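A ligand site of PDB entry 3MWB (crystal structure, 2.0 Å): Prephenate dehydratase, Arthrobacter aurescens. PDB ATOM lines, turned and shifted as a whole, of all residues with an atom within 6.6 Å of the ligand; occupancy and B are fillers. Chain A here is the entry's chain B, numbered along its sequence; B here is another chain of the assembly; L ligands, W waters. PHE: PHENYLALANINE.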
ATOM      1  N   LEU A 208       9.079 -19.630   4.515  1.00  0.00           N
ATOM      2  CA  LEU A 208       9.185 -18.311   3.923  1.00  0.00           C
ATOM      3  C   LEU A 208      10.452 -17.619   4.425  1.00  0.00           C
ATOM      4  O   LEU A 208      10.541 -17.267   5.615  1.00  0.00           O
ATOM      5  CB  LEU A 208       7.943 -17.470   4.269  1.00  0.00           C
ATOM      6  CG  LEU A 208       7.914 -16.048   3.690  1.00  0.00           C
ATOM      7  CD1 LEU A 208       7.670 -16.089   2.192  1.00  0.00           C
ATOM      8  CD2 LEU A 208       6.875 -15.183   4.406  1.00  0.00           C
ATOM      9  N   GLU A 210      11.677 -14.446   3.590  1.00  0.00           N
ATOM     10  CA  GLU A 210      11.434 -13.019   3.903  1.00  0.00           C
ATOM     11  C   GLU A 210       9.984 -12.622   3.638  1.00  0.00           C
ATOM     12  O   GLU A 210       9.419 -12.980   2.601  1.00  0.00           O
ATOM     13  CB  GLU A 210      12.319 -12.092   3.068  1.00  0.00           C
ATOM     14  CG  GLU A 210      13.665 -12.657   2.617  1.00  0.00           C
ATOM     15  CD  GLU A 210      14.554 -11.604   1.996  1.00  0.00           C
ATOM     16  OE1 GLU A 210      14.781 -11.673   0.768  1.00  0.00           O
ATOM     17  OE2 GLU A 210      15.039 -10.712   2.733  1.00  0.00           O
ATOM     18  N   ASP A 211       9.389 -11.849   4.555  1.00  0.00           N
ATOM     19  CA  ASP A 211       7.980 -11.474   4.416  1.00  0.00           C
ATOM     20  C   ASP A 211       7.807 -10.132   3.721  1.00  0.00           C
ATOM     21  O   ASP A 211       8.199  -9.082   4.260  1.00  0.00           O
ATOM     22  CB  ASP A 211       7.253 -11.475   5.759  1.00  0.00           C
ATOM     23  CG  ASP A 211       5.739 -11.496   5.603  1.00  0.00           C
ATOM     24  OD1 ASP A 211       5.252 -12.248   4.737  1.00  0.00           O
ATOM     25  OD2 ASP A 211       5.032 -10.754   6.328  1.00  0.00           O
ATOM     26  N   HIS A 212       7.239 -10.176   2.530  1.00  0.00           N
ATOM     27  CA  HIS A 212       6.993  -8.983   1.715  1.00  0.00           C
ATOM     28  C   HIS A 212       5.930  -9.325   0.667  1.00  0.00           C
ATOM     29  O   HIS A 212       5.700 -10.500   0.411  1.00  0.00           O
ATOM     30  CB  HIS A 212       8.310  -8.442   1.081  1.00  0.00           C
ATOM     31  CG  HIS A 212       9.046  -9.416   0.210  1.00  0.00           C
ATOM     32  ND1 HIS A 212       8.633  -9.742  -1.073  1.00  0.00           N
ATOM     33  CD2 HIS A 212      10.190 -10.121   0.418  1.00  0.00           C
ATOM     34  CE1 HIS A 212       9.469 -10.613  -1.595  1.00  0.00           C
ATOM     35  NE2 HIS A 212      10.422 -10.862  -0.720  1.00  0.00           N
ATOM     36  N   PRO A 213       5.245  -8.305   0.085  1.00  0.00           N
ATOM     37  CA  PRO A 213       4.262  -8.604  -0.966  1.00  0.00           C
ATOM     38  C   PRO A 213       4.868  -9.373  -2.135  1.00  0.00           C
ATOM     39  O   PRO A 213       5.973  -9.059  -2.587  1.00  0.00           O
ATOM     40  CB  PRO A 213       3.847  -7.216  -1.434  1.00  0.00           C
ATOM     41  CG  PRO A 213       3.961  -6.356  -0.196  1.00  0.00           C
ATOM     42  CD  PRO A 213       5.177  -6.900   0.531  1.00  0.00           C
ATOM     43  N   GLY A 214       4.172 -10.387  -2.624  1.00  0.00           N
ATOM     44  CA  GLY A 214       4.706 -11.172  -3.735  1.00  0.00           C
ATOM     45  C   GLY A 214       5.714 -12.244  -3.346  1.00  0.00           C
ATOM     46  O   GLY A 214       6.255 -12.938  -4.218  1.00  0.00           O
ATOM     47  N   ALA A 215       5.973 -12.415  -2.047  1.00  0.00           N
ATOM     48  CA  ALA A 215       6.881 -13.503  -1.603  1.00  0.00           C
ATOM     49  C   ALA A 215       6.270 -14.905  -1.815  1.00  0.00           C
ATOM     50  O   ALA A 215       6.937 -15.835  -2.307  1.00  0.00           O
ATOM     51  CB  ALA A 215       7.304 -13.302  -0.145  1.00  0.00           C
ATOM     52  N   LEU A 216       4.990 -15.061  -1.471  1.00  0.00           N
ATOM     53  CA  LEU A 216       4.273 -16.288  -1.779  1.00  0.00           C
ATOM     54  C   LEU A 216       4.192 -16.507  -3.291  1.00  0.00           C
ATOM     55  O   LEU A 216       4.462 -17.622  -3.772  1.00  0.00           O
ATOM     56  CB  LEU A 216       2.885 -16.322  -1.126  1.00  0.00           C
ATOM     57  CG  LEU A 216       2.057 -17.589  -1.347  1.00  0.00           C
ATOM     58  CD1 LEU A 216       2.836 -18.864  -0.982  1.00  0.00           C
ATOM     59  CD2 LEU A 216       0.726 -17.533  -0.579  1.00  0.00           C
ATOM     60  N   MET A 217       3.829 -15.444  -4.041  1.00  0.00           N
ATOM     61  CA  MET A 217       3.824 -15.465  -5.512  1.00  0.00           C
ATOM     62  C   MET A 217       5.069 -16.153  -6.091  1.00  0.00           C
ATOM     63  O   MET A 217       4.961 -17.011  -6.980  1.00  0.00           O
ATOM     64  CB  MET A 217       3.792 -14.040  -6.074  1.00  0.00           C
ATOM     65  CG  MET A 217       2.539 -13.270  -5.758  1.00  0.00           C
ATOM     66  SD  MET A 217       1.246 -13.491  -7.163  1.00  0.00           S
ATOM     67  CE  MET A 217       2.276 -12.730  -8.649  1.00  0.00           C
ATOM     68  N   SER A 235      -0.945 -21.412   4.826  1.00  0.00           N
ATOM     69  CA  SER A 235       0.119 -20.710   5.525  1.00  0.00           C
ATOM     70  C   SER A 235      -0.015 -20.933   7.044  1.00  0.00           C
ATOM     71  O   SER A 235      -1.127 -21.000   7.589  1.00  0.00           O
ATOM     72  CB  SER A 235       0.064 -19.224   5.209  1.00  0.00           C
ATOM     73  OG  SER A 235      -1.086 -18.643   5.806  1.00  0.00           O
ATOM     74  N   ARG A 236       1.124 -21.033   7.710  1.00  0.00           N
ATOM     75  CA  ARG A 236       1.142 -21.163   9.174  1.00  0.00           C
ATOM     76  C   ARG A 236       2.206 -20.276   9.788  1.00  0.00           C
ATOM     77  O   ARG A 236       3.365 -20.384   9.402  1.00  0.00           O
ATOM     78  CB  ARG A 236       1.448 -22.610   9.538  1.00  0.00           C
ATOM     79  N   GLY A 243      10.954 -15.362   7.617  1.00  0.00           N
ATOM     80  CA  GLY A 243       9.715 -14.653   7.255  1.00  0.00           C
ATOM     81  C   GLY A 243       8.520 -14.997   8.137  1.00  0.00           C
ATOM     82  O   GLY A 243       7.436 -14.425   7.988  1.00  0.00           O
ATOM     83  N   TYR A 245       6.707 -17.772   8.490  1.00  0.00           N
ATOM     84  CA  TYR A 245       5.679 -18.662   7.992  1.00  0.00           C
ATOM     85  C   TYR A 245       6.255 -19.919   7.325  1.00  0.00           C
ATOM     86  O   TYR A 245       7.379 -19.921   6.841  1.00  0.00           O
ATOM     87  CB  TYR A 245       4.788 -17.946   6.970  1.00  0.00           C
ATOM     88  CG  TYR A 245       3.988 -16.756   7.478  1.00  0.00           C
ATOM     89  CD1 TYR A 245       2.721 -16.924   8.056  1.00  0.00           C
ATOM     90  CD2 TYR A 245       4.491 -15.459   7.352  1.00  0.00           C
ATOM     91  CE1 TYR A 245       1.983 -15.801   8.519  1.00  0.00           C
ATOM     92  CE2 TYR A 245       3.759 -14.349   7.818  1.00  0.00           C
ATOM     93  CZ  TYR A 245       2.516 -14.524   8.376  1.00  0.00           C
ATOM     94  OH  TYR A 245       1.827 -13.408   8.840  1.00  0.00           O
ATOM     95  N   PHE A 247       4.537 -22.682   4.373  1.00  0.00           N
ATOM     96  CA  PHE A 247       3.438 -22.965   3.451  1.00  0.00           C
ATOM     97  C   PHE A 247       3.341 -24.472   3.221  1.00  0.00           C
ATOM     98  O   PHE A 247       4.300 -25.104   2.774  1.00  0.00           O
ATOM     99  CB  PHE A 247       3.596 -22.177   2.153  1.00  0.00           C
ATOM    100  CG  PHE A 247       3.604 -20.700   2.354  1.00  0.00           C
ATOM    101  CD1 PHE A 247       2.417 -20.020   2.587  1.00  0.00           C
ATOM    102  CD2 PHE A 247       4.786 -19.984   2.352  1.00  0.00           C
ATOM    103  CE1 PHE A 247       2.423 -18.625   2.790  1.00  0.00           C
ATOM    104  CE2 PHE A 247       4.799 -18.594   2.550  1.00  0.00           C
ATOM    105  CZ  PHE A 247       3.621 -17.929   2.769  1.00  0.00           C
ATOM    106  N   LEU B 220      -3.882 -13.995  -6.213  1.00  0.00           N
ATOM    107  CA  LEU B 220      -2.888 -13.399  -5.317  1.00  0.00           C
ATOM    108  C   LEU B 220      -2.221 -12.137  -5.900  1.00  0.00           C
ATOM    109  O   LEU B 220      -1.921 -11.188  -5.161  1.00  0.00           O
ATOM    110  CB  LEU B 220      -1.864 -14.427  -4.880  1.00  0.00           C
ATOM    111  CG  LEU B 220      -2.468 -15.532  -3.985  1.00  0.00           C
ATOM    112  CD1 LEU B 220      -1.428 -16.189  -3.126  1.00  0.00           C
ATOM    113  CD2 LEU B 220      -3.593 -14.999  -3.089  1.00  0.00           C
ATOM    114  N   PHE B 223      -3.420  -8.609  -4.961  1.00  0.00           N
ATOM    115  CA  PHE B 223      -2.746  -8.039  -3.793  1.00  0.00           C
ATOM    116  C   PHE B 223      -1.272  -7.690  -4.069  1.00  0.00           C
ATOM    117  O   PHE B 223      -0.845  -6.569  -3.797  1.00  0.00           O
ATOM    118  CB  PHE B 223      -2.867  -8.975  -2.583  1.00  0.00           C
ATOM    119  CG  PHE B 223      -4.282  -9.148  -2.076  1.00  0.00           C
ATOM    120  CD1 PHE B 223      -4.959  -8.095  -1.488  1.00  0.00           C
ATOM    121  CD2 PHE B 223      -4.939 -10.370  -2.183  1.00  0.00           C
ATOM    122  CE1 PHE B 223      -6.268  -8.230  -1.027  1.00  0.00           C
ATOM    123  CE2 PHE B 223      -6.240 -10.527  -1.729  1.00  0.00           C
ATOM    124  CZ  PHE B 223      -6.904  -9.464  -1.129  1.00  0.00           C
ATOM    125  N   ALA B 224      -0.507  -8.634  -4.605  1.00  0.00           N
ATOM    126  CA  ALA B 224       0.937  -8.440  -4.771  1.00  0.00           C
ATOM    127  C   ALA B 224       1.291  -7.291  -5.716  1.00  0.00           C
ATOM    128  O   ALA B 224       2.179  -6.497  -5.408  1.00  0.00           O
ATOM    129  CB  ALA B 224       1.630  -9.757  -5.194  1.00  0.00           C
ATOM    130  N   VAL B 228       0.160  -5.064  -1.572  1.00  0.00           N
ATOM    131  CA  VAL B 228      -0.588  -5.513  -0.416  1.00  0.00           C
ATOM    132  C   VAL B 228      -0.050  -6.840   0.105  1.00  0.00           C
ATOM    133  O   VAL B 228      -0.175  -7.876  -0.568  1.00  0.00           O
ATOM    134  CB  VAL B 228      -2.103  -5.660  -0.686  1.00  0.00           C
ATOM    135  CG1 VAL B 228      -2.771  -6.150   0.569  1.00  0.00           C
ATOM    136  CG2 VAL B 228      -2.716  -4.320  -1.117  1.00  0.00           C
ATOM    137  N   ASN B 229       0.525  -6.773   1.304  1.00  0.00           N
ATOM    138  CA  ASN B 229       1.070  -7.911   2.017  1.00  0.00           C
ATOM    139  C   ASN B 229      -0.023  -8.808   2.580  1.00  0.00           C
ATOM    140  O   ASN B 229      -1.028  -8.321   3.146  1.00  0.00           O
ATOM    141  CB  ASN B 229       1.953  -7.399   3.156  1.00  0.00           C
ATOM    142  CG  ASN B 229       2.936  -8.423   3.634  1.00  0.00           C
ATOM    143  OD1 ASN B 229       3.691  -9.000   2.840  1.00  0.00           O
ATOM    144  ND2 ASN B 229       2.953  -8.651   4.925  1.00  0.00           N
ATOM    145  N   LEU B 230       0.202 -10.120   2.481  1.00  0.00           N
ATOM    146  CA  LEU B 230      -0.726 -11.076   3.080  1.00  0.00           C
ATOM    147  C   LEU B 230      -0.203 -11.695   4.376  1.00  0.00           C
ATOM    148  O   LEU B 230       1.020 -11.894   4.539  1.00  0.00           O
ATOM    149  CB  LEU B 230      -1.110 -12.180   2.085  1.00  0.00           C
ATOM    150  CG  LEU B 230      -1.605 -11.734   0.716  1.00  0.00           C
ATOM    151  CD1 LEU B 230      -1.836 -12.982  -0.159  1.00  0.00           C
ATOM    152  CD2 LEU B 230      -2.891 -10.871   0.805  1.00  0.00           C
ATOM    153  N   SER B 231      -1.110 -12.008   5.289  1.00  0.00           N
ATOM    154  CA  SER B 231      -0.725 -12.662   6.544  1.00  0.00           C
ATOM    155  C   SER B 231      -1.363 -14.038   6.714  1.00  0.00           C
ATOM    156  O   SER B 231      -1.010 -14.787   7.639  1.00  0.00           O
ATOM    157  CB  SER B 231      -1.081 -11.765   7.723  1.00  0.00           C
ATOM    158  OG  SER B 231      -2.475 -11.520   7.726  1.00  0.00           O
ATOM    159  N   ARG B 232      -2.327 -14.376   5.842  1.00  0.00           N
ATOM    160  CA  ARG B 232      -2.970 -15.684   5.893  1.00  0.00           C
ATOM    161  C   ARG B 232      -3.562 -16.061   4.561  1.00  0.00           C
ATOM    162  O   ARG B 232      -4.213 -15.244   3.906  1.00  0.00           O
ATOM    163  CB  ARG B 232      -4.057 -15.751   6.972  1.00  0.00           C
ATOM    164  CG  ARG B 232      -4.626 -17.180   7.212  1.00  0.00           C
ATOM    165  CD  ARG B 232      -5.714 -17.180   8.303  1.00  0.00           C
ATOM    166  NE  ARG B 232      -6.798 -16.306   7.874  1.00  0.00           N
ATOM    167  CZ  ARG B 232      -7.847 -16.694   7.153  1.00  0.00           C
ATOM    168  NH1 ARG B 232      -7.992 -17.979   6.826  1.00  0.00           N
ATOM    169  NH2 ARG B 232      -8.759 -15.815   6.768  1.00  0.00           N
ATOM    170  N   ILE B 233      -3.278 -17.289   4.125  1.00  0.00           N
ATOM    171  CA  ILE B 233      -4.057 -17.912   3.047  1.00  0.00           C
ATOM    172  C   ILE B 233      -4.335 -19.384   3.343  1.00  0.00           C
ATOM    173  O   ILE B 233      -3.464 -20.092   3.853  1.00  0.00           O
ATOM    174  CB  ILE B 233      -3.395 -17.771   1.679  1.00  0.00           C
ATOM    175  CG1 ILE B 233      -4.201 -18.550   0.624  1.00  0.00           C
ATOM    176  CG2 ILE B 233      -1.923 -18.217   1.754  1.00  0.00           C
ATOM    177  CD1 ILE B 233      -3.666 -18.470  -0.709  1.00  0.00           C
ATOM    178  N   ASP B 250      -6.230 -13.254   4.565  1.00  0.00           N
ATOM    179  CA  ASP B 250      -6.085 -11.995   5.338  1.00  0.00           C
ATOM    180  C   ASP B 250      -5.021 -11.149   4.662  1.00  0.00           C
ATOM    181  O   ASP B 250      -3.900 -11.655   4.410  1.00  0.00           O
ATOM    182  CB  ASP B 250      -5.678 -12.235   6.804  1.00  0.00           C
ATOM    183  CG  ASP B 250      -6.685 -13.090   7.595  1.00  0.00           C
ATOM    184  OD1 ASP B 250      -7.887 -13.131   7.234  1.00  0.00           O
ATOM    185  OD2 ASP B 250      -6.268 -13.694   8.604  1.00  0.00           O
ATOM    186  N   ASP B 252      -2.932  -7.237   4.749  1.00  0.00           N
ATOM    187  CA  ASP B 252      -2.592  -6.002   5.498  1.00  0.00           C
ATOM    188  C   ASP B 252      -3.271  -4.826   4.832  1.00  0.00           C
ATOM    189  O   ASP B 252      -3.092  -4.594   3.630  1.00  0.00           O
ATOM    190  CB  ASP B 252      -1.097  -5.720   5.443  1.00  0.00           C
ATOM    191  CG  ASP B 252      -0.268  -6.702   6.242  1.00  0.00           C
ATOM    192  OD1 ASP B 252      -0.855  -7.540   6.982  1.00  0.00           O
ATOM    193  OD2 ASP B 252       0.990  -6.601   6.170  1.00  0.00           O
HETATM  194  N   PHE L   1       3.274 -11.697   3.159  1.00  0.00           N
HETATM  195  CA  PHE L   1       3.816 -12.484   1.990  1.00  0.00           C
HETATM  196  C   PHE L   1       2.997 -12.219   0.734  1.00  0.00           C
HETATM  197  O   PHE L   1       3.191 -12.894  -0.314  1.00  0.00           O
HETATM  198  CB  PHE L   1       3.886 -14.014   2.292  1.00  0.00           C
HETATM  199  CG  PHE L   1       2.594 -14.604   2.837  1.00  0.00           C
HETATM  200  CD1 PHE L   1       1.485 -14.848   1.996  1.00  0.00           C
HETATM  201  CD2 PHE L   1       2.499 -14.941   4.203  1.00  0.00           C
HETATM  202  CE1 PHE L   1       0.299 -15.383   2.499  1.00  0.00           C
HETATM  203  CE2 PHE L   1       1.311 -15.497   4.726  1.00  0.00           C
HETATM  204  CZ  PHE L   1       0.205 -15.719   3.865  1.00  0.00           C
HETATM  205  OXT PHE L   1       2.080 -11.357   0.776  1.00  0.00           O
HETATM  206  O   HOH W   1       2.479 -13.244  -2.827  1.00  0.00           O
HETATM  207  O   HOH W   2       1.177  -9.995  -1.512  1.00  0.00           O
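O of the ligand lies within hydrogen-bond range of N of Leu 216, 3.0 Å away. The side-chain amide oxygen (OD1) of Asn 229 of chain B sits at hydrogen-bond distance from a nitrogen (N) of the ligand (2.7 Å). N of Leu 230 of chain B is in hydrogen-bond range of OXT of the ligand, 2.8 Å away. The backbone NH (N) of Ala 215 lies within hydrogen-bond range of an oxygen (O) of the ligand. OD1 of Asp 211 is in salt-bridge range of N of the ligand. A nitrogen (N) of the ligand lies within hydrogen-bond range of the backbone carbonyl oxygen (O) of Leu 230 of chain B (2.7 Å).
The backbone NH (N) of Asp 252 of chain B is in hydrogen-bond range of the backbone carbonyl oxygen (O) of Asn 229 of chain B, at 2.7 Å. The backbone carbonyl oxygen of Tyr 245 sits at hydrogen-bond distance from the backbone NH of Leu 208 (2.9 Å). OD2 of Asp 211 sits at hydrogen-bond distance from ND2 of Asn 229 of chain B. The backbone carbonyl oxygen (O) of Ile 233 of chain B lies within hydrogen-bond range of the backbone NH (N) of Ser 235, at 3.0 Å. The backbone carbonyl oxygen of Ser 231 of chain B sits close to the side-chain hydroxyl of Tyr 245, 3.4 Å away. The backbone carbonyl oxygen (O) of Asp 250 of chain B lies within hydrogen-bond range of the backbone NH (N) of Ser 231 of chain B, 2.9 Å away. The backbone carbonyl oxygen of Leu 208 lies within hydrogen-bond range of the backbone NH of Gly 243, 2.8 Å away. OD1 of Asn 229 of chain B lies close to O of His 212, 3.5 Å away.
Residues that only touch the ligand: His 212, Phe 247, Arg 232 of chain B, Gly 214, Ser 231 of chain B, Ile 233 of chain B, Ser 235, Tyr 245, Leu 208 and Pro 213. Hydrophobic or aromatic side chains within 4 Å of the ligand: Leu 208, Leu 216, Tyr 245, Phe 247, Leu 230 of chain B and Ile 233 of chain B. 15 residues have an atom within 4 Å of the ligand: Leu 208, Asp 211, His 212, Pro 213, Gly 214, Ala 215, Leu 216, Ser 235, Tyr 245, Phe 247, Asn 229 of chain B, Leu 230 of chain B, Ser 231 of chain B, Arg 232 of chain B and Ile 233 of chain B.
Water W2 lies within hydrogen-bond range of the backbone carbonyl oxygen of Val 228 of chain B (2.7 Å), an oxygen (OXT) of the ligand (2.8 Å) and the backbone NH of Gly 214 (3.2 Å).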
